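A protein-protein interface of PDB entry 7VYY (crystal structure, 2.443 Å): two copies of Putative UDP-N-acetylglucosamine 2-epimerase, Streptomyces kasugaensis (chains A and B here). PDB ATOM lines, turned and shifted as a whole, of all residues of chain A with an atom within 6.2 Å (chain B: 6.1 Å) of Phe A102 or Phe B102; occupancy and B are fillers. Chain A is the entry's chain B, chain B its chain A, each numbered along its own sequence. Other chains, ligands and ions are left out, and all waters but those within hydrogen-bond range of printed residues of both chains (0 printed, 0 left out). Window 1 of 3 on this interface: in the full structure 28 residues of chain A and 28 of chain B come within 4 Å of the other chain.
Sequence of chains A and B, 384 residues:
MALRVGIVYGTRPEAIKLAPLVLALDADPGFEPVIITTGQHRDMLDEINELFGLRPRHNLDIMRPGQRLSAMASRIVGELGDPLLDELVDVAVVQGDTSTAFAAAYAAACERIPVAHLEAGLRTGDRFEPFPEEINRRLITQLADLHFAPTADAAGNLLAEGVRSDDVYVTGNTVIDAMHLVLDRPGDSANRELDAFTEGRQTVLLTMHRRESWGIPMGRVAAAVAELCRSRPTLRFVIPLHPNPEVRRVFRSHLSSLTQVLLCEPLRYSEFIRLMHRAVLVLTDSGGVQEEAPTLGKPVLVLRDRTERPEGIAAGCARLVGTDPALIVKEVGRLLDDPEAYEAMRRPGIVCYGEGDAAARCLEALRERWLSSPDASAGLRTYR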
ATOM      1  N   ALA A  73     -36.846  -8.115   5.920  1.00  0.00           N
ATOM      2  CA  ALA A  73     -35.743  -8.623   5.067  1.00  0.00           C
ATOM      3  C   ALA A  73     -36.289  -9.005   3.684  1.00  0.00           C
ATOM      4  O   ALA A  73     -35.669  -8.618   2.668  1.00  0.00           O
ATOM      5  CB  ALA A  73     -35.068  -9.790   5.740  1.00  0.00           C
ATOM      6  N   VAL A  77     -35.149  -7.214   0.299  1.00  0.00           N
ATOM      7  CA  VAL A  77     -34.445  -8.116  -0.660  1.00  0.00           C
ATOM      8  C   VAL A  77     -35.226  -8.151  -1.976  1.00  0.00           C
ATOM      9  O   VAL A  77     -34.574  -8.223  -3.033  1.00  0.00           O
ATOM     10  CB  VAL A  77     -34.235  -9.520  -0.067  1.00  0.00           C
ATOM     11  CG1 VAL A  77     -33.877 -10.551  -1.126  1.00  0.00           C
ATOM     12  CG2 VAL A  77     -33.182  -9.489   1.030  1.00  0.00           C
ATOM     13  N   VAL A  94     -23.929   0.946   2.545  1.00  0.00           N
ATOM     14  CA  VAL A  94     -24.801   0.677   3.731  1.00  0.00           C
ATOM     15  C   VAL A  94     -24.002   0.997   4.997  1.00  0.00           C
ATOM     16  O   VAL A  94     -22.762   1.056   4.911  1.00  0.00           O
ATOM     17  CB  VAL A  94     -25.356  -0.761   3.750  1.00  0.00           C
ATOM     18  CG1 VAL A  94     -26.247  -1.027   2.550  1.00  0.00           C
ATOM     19  CG2 VAL A  94     -24.256  -1.803   3.850  1.00  0.00           C
ATOM     20  N   ASP A  97     -24.971  -1.975  11.608  1.00  0.00           N
ATOM     21  CA  ASP A  97     -25.279  -3.392  11.942  1.00  0.00           C
ATOM     22  C   ASP A  97     -26.769  -3.672  11.745  1.00  0.00           C
ATOM     23  O   ASP A  97     -27.248  -4.701  12.251  1.00  0.00           O
ATOM     24  CB  ASP A  97     -24.854  -3.703  13.381  1.00  0.00           C
ATOM     25  CG  ASP A  97     -25.399  -2.720  14.405  1.00  0.00           C
ATOM     26  OD1 ASP A  97     -26.396  -2.049  14.100  1.00  0.00           O
ATOM     27  OD2 ASP A  97     -24.828  -2.636  15.503  1.00  0.00           O
ATOM     28  N   THR A  98     -27.470  -2.794  11.028  1.00  0.00           N
ATOM     29  CA  THR A  98     -28.948  -2.829  10.880  1.00  0.00           C
ATOM     30  C   THR A  98     -29.327  -3.974   9.942  1.00  0.00           C
ATOM     31  O   THR A  98     -28.461  -4.442   9.180  1.00  0.00           O
ATOM     32  CB  THR A  98     -29.501  -1.491  10.368  1.00  0.00           C
ATOM     33  OG1 THR A  98     -28.857  -1.154   9.136  1.00  0.00           O
ATOM     34  CG2 THR A  98     -29.300  -0.369  11.364  1.00  0.00           C
ATOM     35  N   SER A  99     -30.585  -4.391  10.000  1.00  0.00           N
ATOM     36  CA  SER A  99     -31.167  -5.432   9.117  1.00  0.00           C
ATOM     37  C   SER A  99     -31.383  -4.838   7.724  1.00  0.00           C
ATOM     38  O   SER A  99     -31.300  -5.607   6.758  1.00  0.00           O
ATOM     39  CB  SER A  99     -32.439  -5.988   9.707  1.00  0.00           C
ATOM     40  OG  SER A  99     -32.171  -6.607  10.954  1.00  0.00           O
ATOM     41  N   THR A 100     -31.628  -3.524   7.640  1.00  0.00           N
ATOM     42  CA  THR A 100     -31.645  -2.741   6.371  1.00  0.00           C
ATOM     43  C   THR A 100     -30.302  -2.934   5.662  1.00  0.00           C
ATOM     44  O   THR A 100     -30.304  -3.467   4.550  1.00  0.00           O
ATOM     45  CB  THR A 100     -31.936  -1.251   6.609  1.00  0.00           C
ATOM     46  OG1 THR A 100     -33.259  -1.129   7.123  1.00  0.00           O
ATOM     47  CG2 THR A 100     -31.833  -0.402   5.358  1.00  0.00           C
ATOM     48  N   ALA A 101     -29.206  -2.556   6.322  1.00  0.00           N
ATOM     49  CA  ALA A 101     -27.829  -2.604   5.782  1.00  0.00           C
ATOM     50  C   ALA A 101     -27.521  -3.996   5.220  1.00  0.00           C
ATOM     51  O   ALA A 101     -26.877  -4.066   4.142  1.00  0.00           O
ATOM     52  CB  ALA A 101     -26.826  -2.197   6.837  1.00  0.00           C
ATOM     53  N   PHE A 102     -27.930  -5.066   5.911  1.00  0.00           N
ATOM     54  CA  PHE A 102     -27.696  -6.458   5.437  1.00  0.00           C
ATOM     55  C   PHE A 102     -28.589  -6.741   4.226  1.00  0.00           C
ATOM     56  O   PHE A 102     -28.072  -7.212   3.202  1.00  0.00           O
ATOM     57  CB  PHE A 102     -27.948  -7.525   6.499  1.00  0.00           C
ATOM     58  CG  PHE A 102     -28.287  -8.859   5.886  1.00  0.00           C
ATOM     59  CD1 PHE A 102     -27.336  -9.564   5.167  1.00  0.00           C
ATOM     60  CD2 PHE A 102     -29.574  -9.382   5.967  1.00  0.00           C
ATOM     61  CE1 PHE A 102     -27.655 -10.776   4.572  1.00  0.00           C
ATOM     62  CE2 PHE A 102     -29.890 -10.590   5.366  1.00  0.00           C
ATOM     63  CZ  PHE A 102     -28.932 -11.281   4.671  1.00  0.00           C
ATOM     64  N   ALA A 103     -29.893  -6.489   4.349  1.00  0.00           N
ATOM     65  CA  ALA A 103     -30.894  -6.809   3.304  1.00  0.00           C
ATOM     66  C   ALA A 103     -30.569  -6.012   2.033  1.00  0.00           C
ATOM     67  O   ALA A 103     -30.610  -6.599   0.922  1.00  0.00           O
ATOM     68  CB  ALA A 103     -32.282  -6.532   3.818  1.00  0.00           C
ATOM     69  N   ALA A 104     -30.230  -4.732   2.197  1.00  0.00           N
ATOM     70  CA  ALA A 104     -29.819  -3.801   1.117  1.00  0.00           C
ATOM     71  C   ALA A 104     -28.585  -4.352   0.393  1.00  0.00           C
ATOM     72  O   ALA A 104     -28.617  -4.426  -0.844  1.00  0.00           O
ATOM     73  CB  ALA A 104     -29.549  -2.435   1.685  1.00  0.00           C
ATOM     74  N   ALA A 105     -27.556  -4.753   1.147  1.00  0.00           N
ATOM     75  CA  ALA A 105     -26.292  -5.317   0.616  1.00  0.00           C
ATOM     76  C   ALA A 105     -26.563  -6.583  -0.207  1.00  0.00           C
ATOM     77  O   ALA A 105     -25.979  -6.716  -1.304  1.00  0.00           O
ATOM     78  CB  ALA A 105     -25.327  -5.593   1.737  1.00  0.00           C
ATOM     79  N   TYR A 106     -27.398  -7.499   0.289  1.00  0.00           N
ATOM     80  CA  TYR A 106     -27.753  -8.735  -0.461  1.00  0.00           C
ATOM     81  C   TYR A 106     -28.475  -8.359  -1.766  1.00  0.00           C
ATOM     82  O   TYR A 106     -28.175  -8.986  -2.808  1.00  0.00           O
ATOM     83  CB  TYR A 106     -28.601  -9.706   0.364  1.00  0.00           C
ATOM     84  CG  TYR A 106     -28.922 -10.963  -0.405  1.00  0.00           C
ATOM     85  CD1 TYR A 106     -27.948 -11.919  -0.611  1.00  0.00           C
ATOM     86  CD2 TYR A 106     -30.158 -11.162  -1.001  1.00  0.00           C
ATOM     87  CE1 TYR A 106     -28.200 -13.070  -1.334  1.00  0.00           C
ATOM     88  CE2 TYR A 106     -30.423 -12.295  -1.753  1.00  0.00           C
ATOM     89  CZ  TYR A 106     -29.443 -13.260  -1.906  1.00  0.00           C
ATOM     90  OH  TYR A 106     -29.681 -14.396  -2.616  1.00  0.00           O
ATOM     91  N   ALA A 107     -29.394  -7.385  -1.709  1.00  0.00           N
ATOM     92  CA  ALA A 107     -30.193  -6.908  -2.865  1.00  0.00           C
ATOM     93  C   ALA A 107     -29.259  -6.340  -3.940  1.00  0.00           C
ATOM     94  O   ALA A 107     -29.385  -6.740  -5.121  1.00  0.00           O
ATOM     95  CB  ALA A 107     -31.194  -5.879  -2.409  1.00  0.00           C
ATOM     96  N   ASN A 136     -25.753  -9.732  11.538  1.00  0.00           N
ATOM     97  CA  ASN A 136     -25.834  -8.710  10.464  1.00  0.00           C
ATOM     98  C   ASN A 136     -24.428  -8.216  10.114  1.00  0.00           C
ATOM     99  O   ASN A 136     -24.081  -8.205   8.928  1.00  0.00           O
ATOM    100  CB  ASN A 136     -26.723  -7.533  10.878  1.00  0.00           C
ATOM    101  CG  ASN A 136     -28.200  -7.843  10.784  1.00  0.00           C
ATOM    102  OD1 ASN A 136     -28.602  -8.798  10.119  1.00  0.00           O
ATOM    103  ND2 ASN A 136     -29.015  -7.013  11.415  1.00  0.00           N
ATOM    104  N   LEU A 139     -22.587 -10.887   8.209  1.00  0.00           N
ATOM    105  CA  LEU A 139     -23.184 -11.089   6.866  1.00  0.00           C
ATOM    106  C   LEU A 139     -22.743  -9.942   5.941  1.00  0.00           C
ATOM    107  O   LEU A 139     -22.267 -10.240   4.810  1.00  0.00           O
ATOM    108  CB  LEU A 139     -24.707 -11.170   6.984  1.00  0.00           C
ATOM    109  CG  LEU A 139     -25.255 -12.418   7.667  1.00  0.00           C
ATOM    110  CD1 LEU A 139     -26.761 -12.305   7.860  1.00  0.00           C
ATOM    111  CD2 LEU A 139     -24.905 -13.685   6.903  1.00  0.00           C
ATOM    112  N   ILE A 140     -22.911  -8.688   6.385  1.00  0.00           N
ATOM    113  CA  ILE A 140     -22.553  -7.467   5.603  1.00  0.00           C
ATOM    114  C   ILE A 140     -21.070  -7.563   5.219  1.00  0.00           C
ATOM    115  O   ILE A 140     -20.736  -7.269   4.050  1.00  0.00           O
ATOM    116  CB  ILE A 140     -22.865  -6.177   6.384  1.00  0.00           C
ATOM    117  CG1 ILE A 140     -24.367  -5.976   6.575  1.00  0.00           C
ATOM    118  CG2 ILE A 140     -22.246  -4.967   5.696  1.00  0.00           C
ATOM    119  CD1 ILE A 140     -24.728  -5.060   7.724  1.00  0.00           C
ATOM    120  N   LEU A 143     -20.482  -9.625   2.218  1.00  0.00           N
ATOM    121  CA  LEU A 143     -21.124  -9.089   0.990  1.00  0.00           C
ATOM    122  C   LEU A 143     -20.337  -7.897   0.439  1.00  0.00           C
ATOM    123  O   LEU A 143     -20.344  -7.713  -0.789  1.00  0.00           O
ATOM    124  CB  LEU A 143     -22.569  -8.690   1.300  1.00  0.00           C
ATOM    125  CG  LEU A 143     -23.556  -9.850   1.363  1.00  0.00           C
ATOM    126  CD1 LEU A 143     -24.877  -9.396   1.952  1.00  0.00           C
ATOM    127  CD2 LEU A 143     -23.771 -10.453  -0.016  1.00  0.00           C
ATOM    128  N   ALA B  73     -35.001 -15.439  -3.269  1.00  0.00           N
ATOM    129  CA  ALA B  73     -34.495 -15.165  -1.905  1.00  0.00           C
ATOM    130  C   ALA B  73     -35.608 -14.538  -1.051  1.00  0.00           C
ATOM    131  O   ALA B  73     -35.800 -14.977   0.104  1.00  0.00           O
ATOM    132  CB  ALA B  73     -33.283 -14.281  -1.967  1.00  0.00           C
ATOM    133  N   VAL B  77     -37.092 -16.240   2.231  1.00  0.00           N
ATOM    134  CA  VAL B  77     -36.843 -15.469   3.486  1.00  0.00           C
ATOM    135  C   VAL B  77     -38.191 -15.121   4.132  1.00  0.00           C
ATOM    136  O   VAL B  77     -38.252 -15.122   5.374  1.00  0.00           O
ATOM    137  CB  VAL B  77     -35.988 -14.210   3.246  1.00  0.00           C
ATOM    138  CG1 VAL B  77     -36.010 -13.262   4.438  1.00  0.00           C
ATOM    139  CG2 VAL B  77     -34.552 -14.572   2.912  1.00  0.00           C
ATOM    140  N   VAL B  94     -29.307 -27.170   6.123  1.00  0.00           N
ATOM    141  CA  VAL B  94     -29.225 -26.783   4.682  1.00  0.00           C
ATOM    142  C   VAL B  94     -27.950 -27.398   4.082  1.00  0.00           C
ATOM    143  O   VAL B  94     -27.062 -27.798   4.852  1.00  0.00           O
ATOM    144  CB  VAL B  94     -29.272 -25.259   4.482  1.00  0.00           C
ATOM    145  CG1 VAL B  94     -30.580 -24.668   4.981  1.00  0.00           C
ATOM    146  CG2 VAL B  94     -28.087 -24.548   5.106  1.00  0.00           C
ATOM    147  N   ASP B  97     -24.151 -24.849  -1.620  1.00  0.00           N
ATOM    148  CA  ASP B  97     -23.857 -23.431  -1.950  1.00  0.00           C
ATOM    149  C   ASP B  97     -25.074 -22.787  -2.616  1.00  0.00           C
ATOM    150  O   ASP B  97     -24.904 -21.710  -3.222  1.00  0.00           O
ATOM    151  CB  ASP B  97     -22.624 -23.342  -2.850  1.00  0.00           C
ATOM    152  CG  ASP B  97     -22.704 -24.211  -4.093  1.00  0.00           C
ATOM    153  OD1 ASP B  97     -23.826 -24.609  -4.471  1.00  0.00           O
ATOM    154  OD2 ASP B  97     -21.638 -24.490  -4.674  1.00  0.00           O
ATOM    155  N   THR B  98     -26.253 -23.409  -2.498  1.00  0.00           N
ATOM    156  CA  THR B  98     -27.482 -22.997  -3.232  1.00  0.00           C
ATOM    157  C   THR B  98     -28.028 -21.718  -2.612  1.00  0.00           C
ATOM    158  O   THR B  98     -27.665 -21.419  -1.470  1.00  0.00           O
ATOM    159  CB  THR B  98     -28.553 -24.095  -3.250  1.00  0.00           C
ATOM    160  OG1 THR B  98     -28.874 -24.477  -1.911  1.00  0.00           O
ATOM    161  CG2 THR B  98     -28.116 -25.314  -4.032  1.00  0.00           C
ATOM    162  N   SER B  99     -28.869 -21.005  -3.358  1.00  0.00           N
ATOM    163  CA  SER B  99     -29.551 -19.770  -2.894  1.00  0.00           C
ATOM    164  C   SER B  99     -30.666 -20.156  -1.921  1.00  0.00           C
ATOM    165  O   SER B  99     -30.957 -19.344  -1.031  1.00  0.00           O
ATOM    166  CB  SER B  99     -30.052 -18.955  -4.052  1.00  0.00           C
ATOM    167  OG  SER B  99     -28.960 -18.562  -4.875  1.00  0.00           O
ATOM    168  N   THR B 100     -31.243 -21.355  -2.083  1.00  0.00           N
ATOM    169  CA  THR B 100     -32.195 -21.977  -1.121  1.00  0.00           C
ATOM    170  C   THR B 100     -31.499 -22.070   0.242  1.00  0.00           C
ATOM    171  O   THR B 100     -31.994 -21.441   1.196  1.00  0.00           O
ATOM    172  CB  THR B 100     -32.688 -23.350  -1.602  1.00  0.00           C
ATOM    173  OG1 THR B 100     -33.453 -23.185  -2.798  1.00  0.00           O
ATOM    174  CG2 THR B 100     -33.557 -24.069  -0.596  1.00  0.00           C
ATOM    175  N   ALA B 101     -30.370 -22.784   0.301  1.00  0.00           N
ATOM    176  CA  ALA B 101     -29.585 -23.042   1.529  1.00  0.00           C
ATOM    177  C   ALA B 101     -29.285 -21.733   2.260  1.00  0.00           C
ATOM    178  O   ALA B 101     -29.372 -21.734   3.507  1.00  0.00           O
ATOM    179  CB  ALA B 101     -28.308 -23.781   1.205  1.00  0.00           C
ATOM    180  N   PHE B 102     -28.924 -20.668   1.534  1.00  0.00           N
ATOM    181  CA  PHE B 102     -28.627 -19.345   2.145  1.00  0.00           C
ATOM    182  C   PHE B 102     -29.922 -18.722   2.656  1.00  0.00           C
ATOM    183  O   PHE B 102     -29.950 -18.306   3.822  1.00  0.00           O
ATOM    184  CB  PHE B 102     -27.942 -18.359   1.194  1.00  0.00           C
ATOM    185  CG  PHE B 102     -28.192 -16.924   1.579  1.00  0.00           C
ATOM    186  CD1 PHE B 102     -27.674 -16.404   2.753  1.00  0.00           C
ATOM    187  CD2 PHE B 102     -29.007 -16.114   0.808  1.00  0.00           C
ATOM    188  CE1 PHE B 102     -27.952 -15.102   3.140  1.00  0.00           C
ATOM    189  CE2 PHE B 102     -29.287 -14.809   1.195  1.00  0.00           C
ATOM    190  CZ  PHE B 102     -28.753 -14.305   2.357  1.00  0.00           C
ATOM    191  N   ALA B 103     -30.942 -18.620   1.801  1.00  0.00           N
ATOM    192  CA  ALA B 103     -32.221 -17.948   2.130  1.00  0.00           C
ATOM    193  C   ALA B 103     -32.898 -18.678   3.300  1.00  0.00           C
ATOM    194  O   ALA B 103     -33.392 -17.999   4.227  1.00  0.00           O
ATOM    195  CB  ALA B 103     -33.094 -17.903   0.908  1.00  0.00           C
ATOM    196  N   ALA B 104     -32.890 -20.016   3.261  1.00  0.00           N
ATOM    197  CA  ALA B 104     -33.419 -20.916   4.316  1.00  0.00           C
ATOM    198  C   ALA B 104     -32.698 -20.641   5.642  1.00  0.00           C
ATOM    199  O   ALA B 104     -33.390 -20.472   6.650  1.00  0.00           O
ATOM    200  CB  ALA B 104     -33.264 -22.359   3.898  1.00  0.00           C
ATOM    201  N   ALA B 105     -31.363 -20.572   5.629  1.00  0.00           N
ATOM    202  CA  ALA B 105     -30.516 -20.351   6.828  1.00  0.00           C
ATOM    203  C   ALA B 105     -30.825 -18.985   7.444  1.00  0.00           C
ATOM    204  O   ALA B 105     -30.937 -18.902   8.687  1.00  0.00           O
ATOM    205  CB  ALA B 105     -29.057 -20.471   6.487  1.00  0.00           C
ATOM    206  N   TYR B 106     -30.971 -17.943   6.629  1.00  0.00           N
ATOM    207  CA  TYR B 106     -31.340 -16.598   7.138  1.00  0.00           C
ATOM    208  C   TYR B 106     -32.739 -16.645   7.767  1.00  0.00           C
ATOM    209  O   TYR B 106     -32.930 -16.029   8.825  1.00  0.00           O
ATOM    210  CB  TYR B 106     -31.250 -15.518   6.063  1.00  0.00           C
ATOM    211  CG  TYR B 106     -31.561 -14.158   6.624  1.00  0.00           C
ATOM    212  CD1 TYR B 106     -30.677 -13.521   7.482  1.00  0.00           C
ATOM    213  CD2 TYR B 106     -32.776 -13.551   6.378  1.00  0.00           C
ATOM    214  CE1 TYR B 106     -30.977 -12.295   8.052  1.00  0.00           C
ATOM    215  CE2 TYR B 106     -33.091 -12.320   6.933  1.00  0.00           C
ATOM    216  CZ  TYR B 106     -32.188 -11.689   7.770  1.00  0.00           C
ATOM    217  OH  TYR B 106     -32.485 -10.481   8.333  1.00  0.00           O
ATOM    218  N   ALA B 107     -33.686 -17.343   7.136  1.00  0.00           N
ATOM    219  CA  ALA B 107     -35.089 -17.501   7.608  1.00  0.00           C
ATOM    220  C   ALA B 107     -35.100 -18.197   8.979  1.00  0.00           C
ATOM    221  O   ALA B 107     -35.753 -17.698   9.896  1.00  0.00           O
ATOM    222  CB  ALA B 107     -35.904 -18.272   6.595  1.00  0.00           C
ATOM    223  N   ASN B 136     -22.818 -17.191  -1.374  1.00  0.00           N
ATOM    224  CA  ASN B 136     -23.768 -18.063  -0.624  1.00  0.00           C
ATOM    225  C   ASN B 136     -22.989 -18.876   0.420  1.00  0.00           C
ATOM    226  O   ASN B 136     -23.377 -18.857   1.591  1.00  0.00           O
ATOM    227  CB  ASN B 136     -24.552 -19.004  -1.548  1.00  0.00           C
ATOM    228  CG  ASN B 136     -25.664 -18.324  -2.321  1.00  0.00           C
ATOM    229  OD1 ASN B 136     -26.081 -17.211  -2.000  1.00  0.00           O
ATOM    230  ND2 ASN B 136     -26.147 -18.982  -3.360  1.00  0.00           N
ATOM    231  N   LEU B 139     -21.902 -16.605   3.248  1.00  0.00           N
ATOM    232  CA  LEU B 139     -23.073 -16.153   4.035  1.00  0.00           C
ATOM    233  C   LEU B 139     -23.557 -17.298   4.942  1.00  0.00           C
ATOM    234  O   LEU B 139     -23.718 -17.058   6.153  1.00  0.00           O
ATOM    235  CB  LEU B 139     -24.166 -15.666   3.080  1.00  0.00           C
ATOM    236  CG  LEU B 139     -23.867 -14.335   2.395  1.00  0.00           C
ATOM    237  CD1 LEU B 139     -24.906 -14.009   1.338  1.00  0.00           C
ATOM    238  CD2 LEU B 139     -23.814 -13.217   3.421  1.00  0.00           C
ATOM    239  N   ILE B 140     -23.774 -18.490   4.379  1.00  0.00           N
ATOM    240  CA  ILE B 140     -24.253 -19.696   5.117  1.00  0.00           C
ATOM    241  C   ILE B 140     -23.284 -19.955   6.283  1.00  0.00           C
ATOM    242  O   ILE B 140     -23.760 -20.247   7.402  1.00  0.00           O
ATOM    243  CB  ILE B 140     -24.391 -20.916   4.181  1.00  0.00           C
ATOM    244  CG1 ILE B 140     -25.527 -20.741   3.167  1.00  0.00           C
ATOM    245  CG2 ILE B 140     -24.576 -22.193   4.988  1.00  0.00           C
ATOM    246  CD1 ILE B 140     -25.400 -21.630   1.940  1.00  0.00           C
ATOM    247  N   LEU B 143     -23.999 -17.891   9.238  1.00  0.00           N
ATOM    248  CA  LEU B 143     -25.351 -18.131   9.809  1.00  0.00           C
ATOM    249  C   LEU B 143     -25.360 -19.439  10.608  1.00  0.00           C
ATOM    250  O   LEU B 143     -26.118 -19.524  11.584  1.00  0.00           O
ATOM    251  CB  LEU B 143     -26.393 -18.153   8.685  1.00  0.00           C
ATOM    252  CG  LEU B 143     -26.771 -16.791   8.109  1.00  0.00           C
ATOM    253  CD1 LEU B 143     -27.559 -16.928   6.809  1.00  0.00           C
ATOM    254  CD2 LEU B 143     -27.555 -15.969   9.106  1.00  0.00           C
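Of the 18 printed residues of chain A, 6 touch a printed residue of chain B.
Printed residues of chain A that touch a printed residue of chain B: Ala A73, Val A77, Phe A102, Tyr A106, Leu A139 and Leu A143.
Of the 18 printed residues of chain B, 6 touch a printed residue of chain A.
Hydrophobic or aromatic side chains of chain B within 4 Å of the printed part of chain A: Ala B73, Val B77, Phe B102, Tyr B106, Leu B139 and Leu B143.
Among the printed residues, no Asp or Glu carboxylate lies within 4 Å of a Lys or Arg side-chain nitrogen of the other chain.
Val B77 touches Ala A73 (CG1 to CB, 3.8 Å).
CE2 of Tyr B106 touches CB of Ala A73, at 3.4 Å.
Ala B73 touches Val A77.
CZ of Phe A102 touches CZ of Phe B102, 3.8 Å away.
Tyr B106 touches Phe A102.
Tyr A106 touches Ala B73 (CE2 to CB, 3.5 Å).
Phe B102 touches Tyr A106.
Leu A139 touches Leu B139 (O to CD2, 3.6 Å).
Leu A139 touches Leu B143.
Leu A143 touches Leu B139.
Ala A73 touches Tyr B106, and with the chains exchanged Tyr A106 touches Ala B73.
Phe A102 touches its own counterpart, Phe B102.
Leu B139 touches its own counterpart, Leu A139.
Leu A139 touches Leu B143, and with the chains exchanged Leu A143 touches Leu B139.
18 positions are printed for both chains.
Of chain B, only Phe B102 and Tyr B106 come within 4 Å of Phe A102.
Phe B102 touches just these residues of chain A: Phe A102 and Tyr A106.
Of the printed residues of chain A, Leu B143 touches Leu A139.
Printed residues of chain A within 4 Å of Tyr B106: Ala A73 (3.4 Å) and Phe A102 (3.4 Å).
Printed residues of chain B within 4 Å of Val A77: Ala B73.
Of the printed residues of chain B, Leu A143 touches Leu B139 (3.95 Å).
Ile A140 touches none of the printed residues of chain B.
The nearest residue of chain B that does not touch Phe A102 is Leu B139 (4.7 Å).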
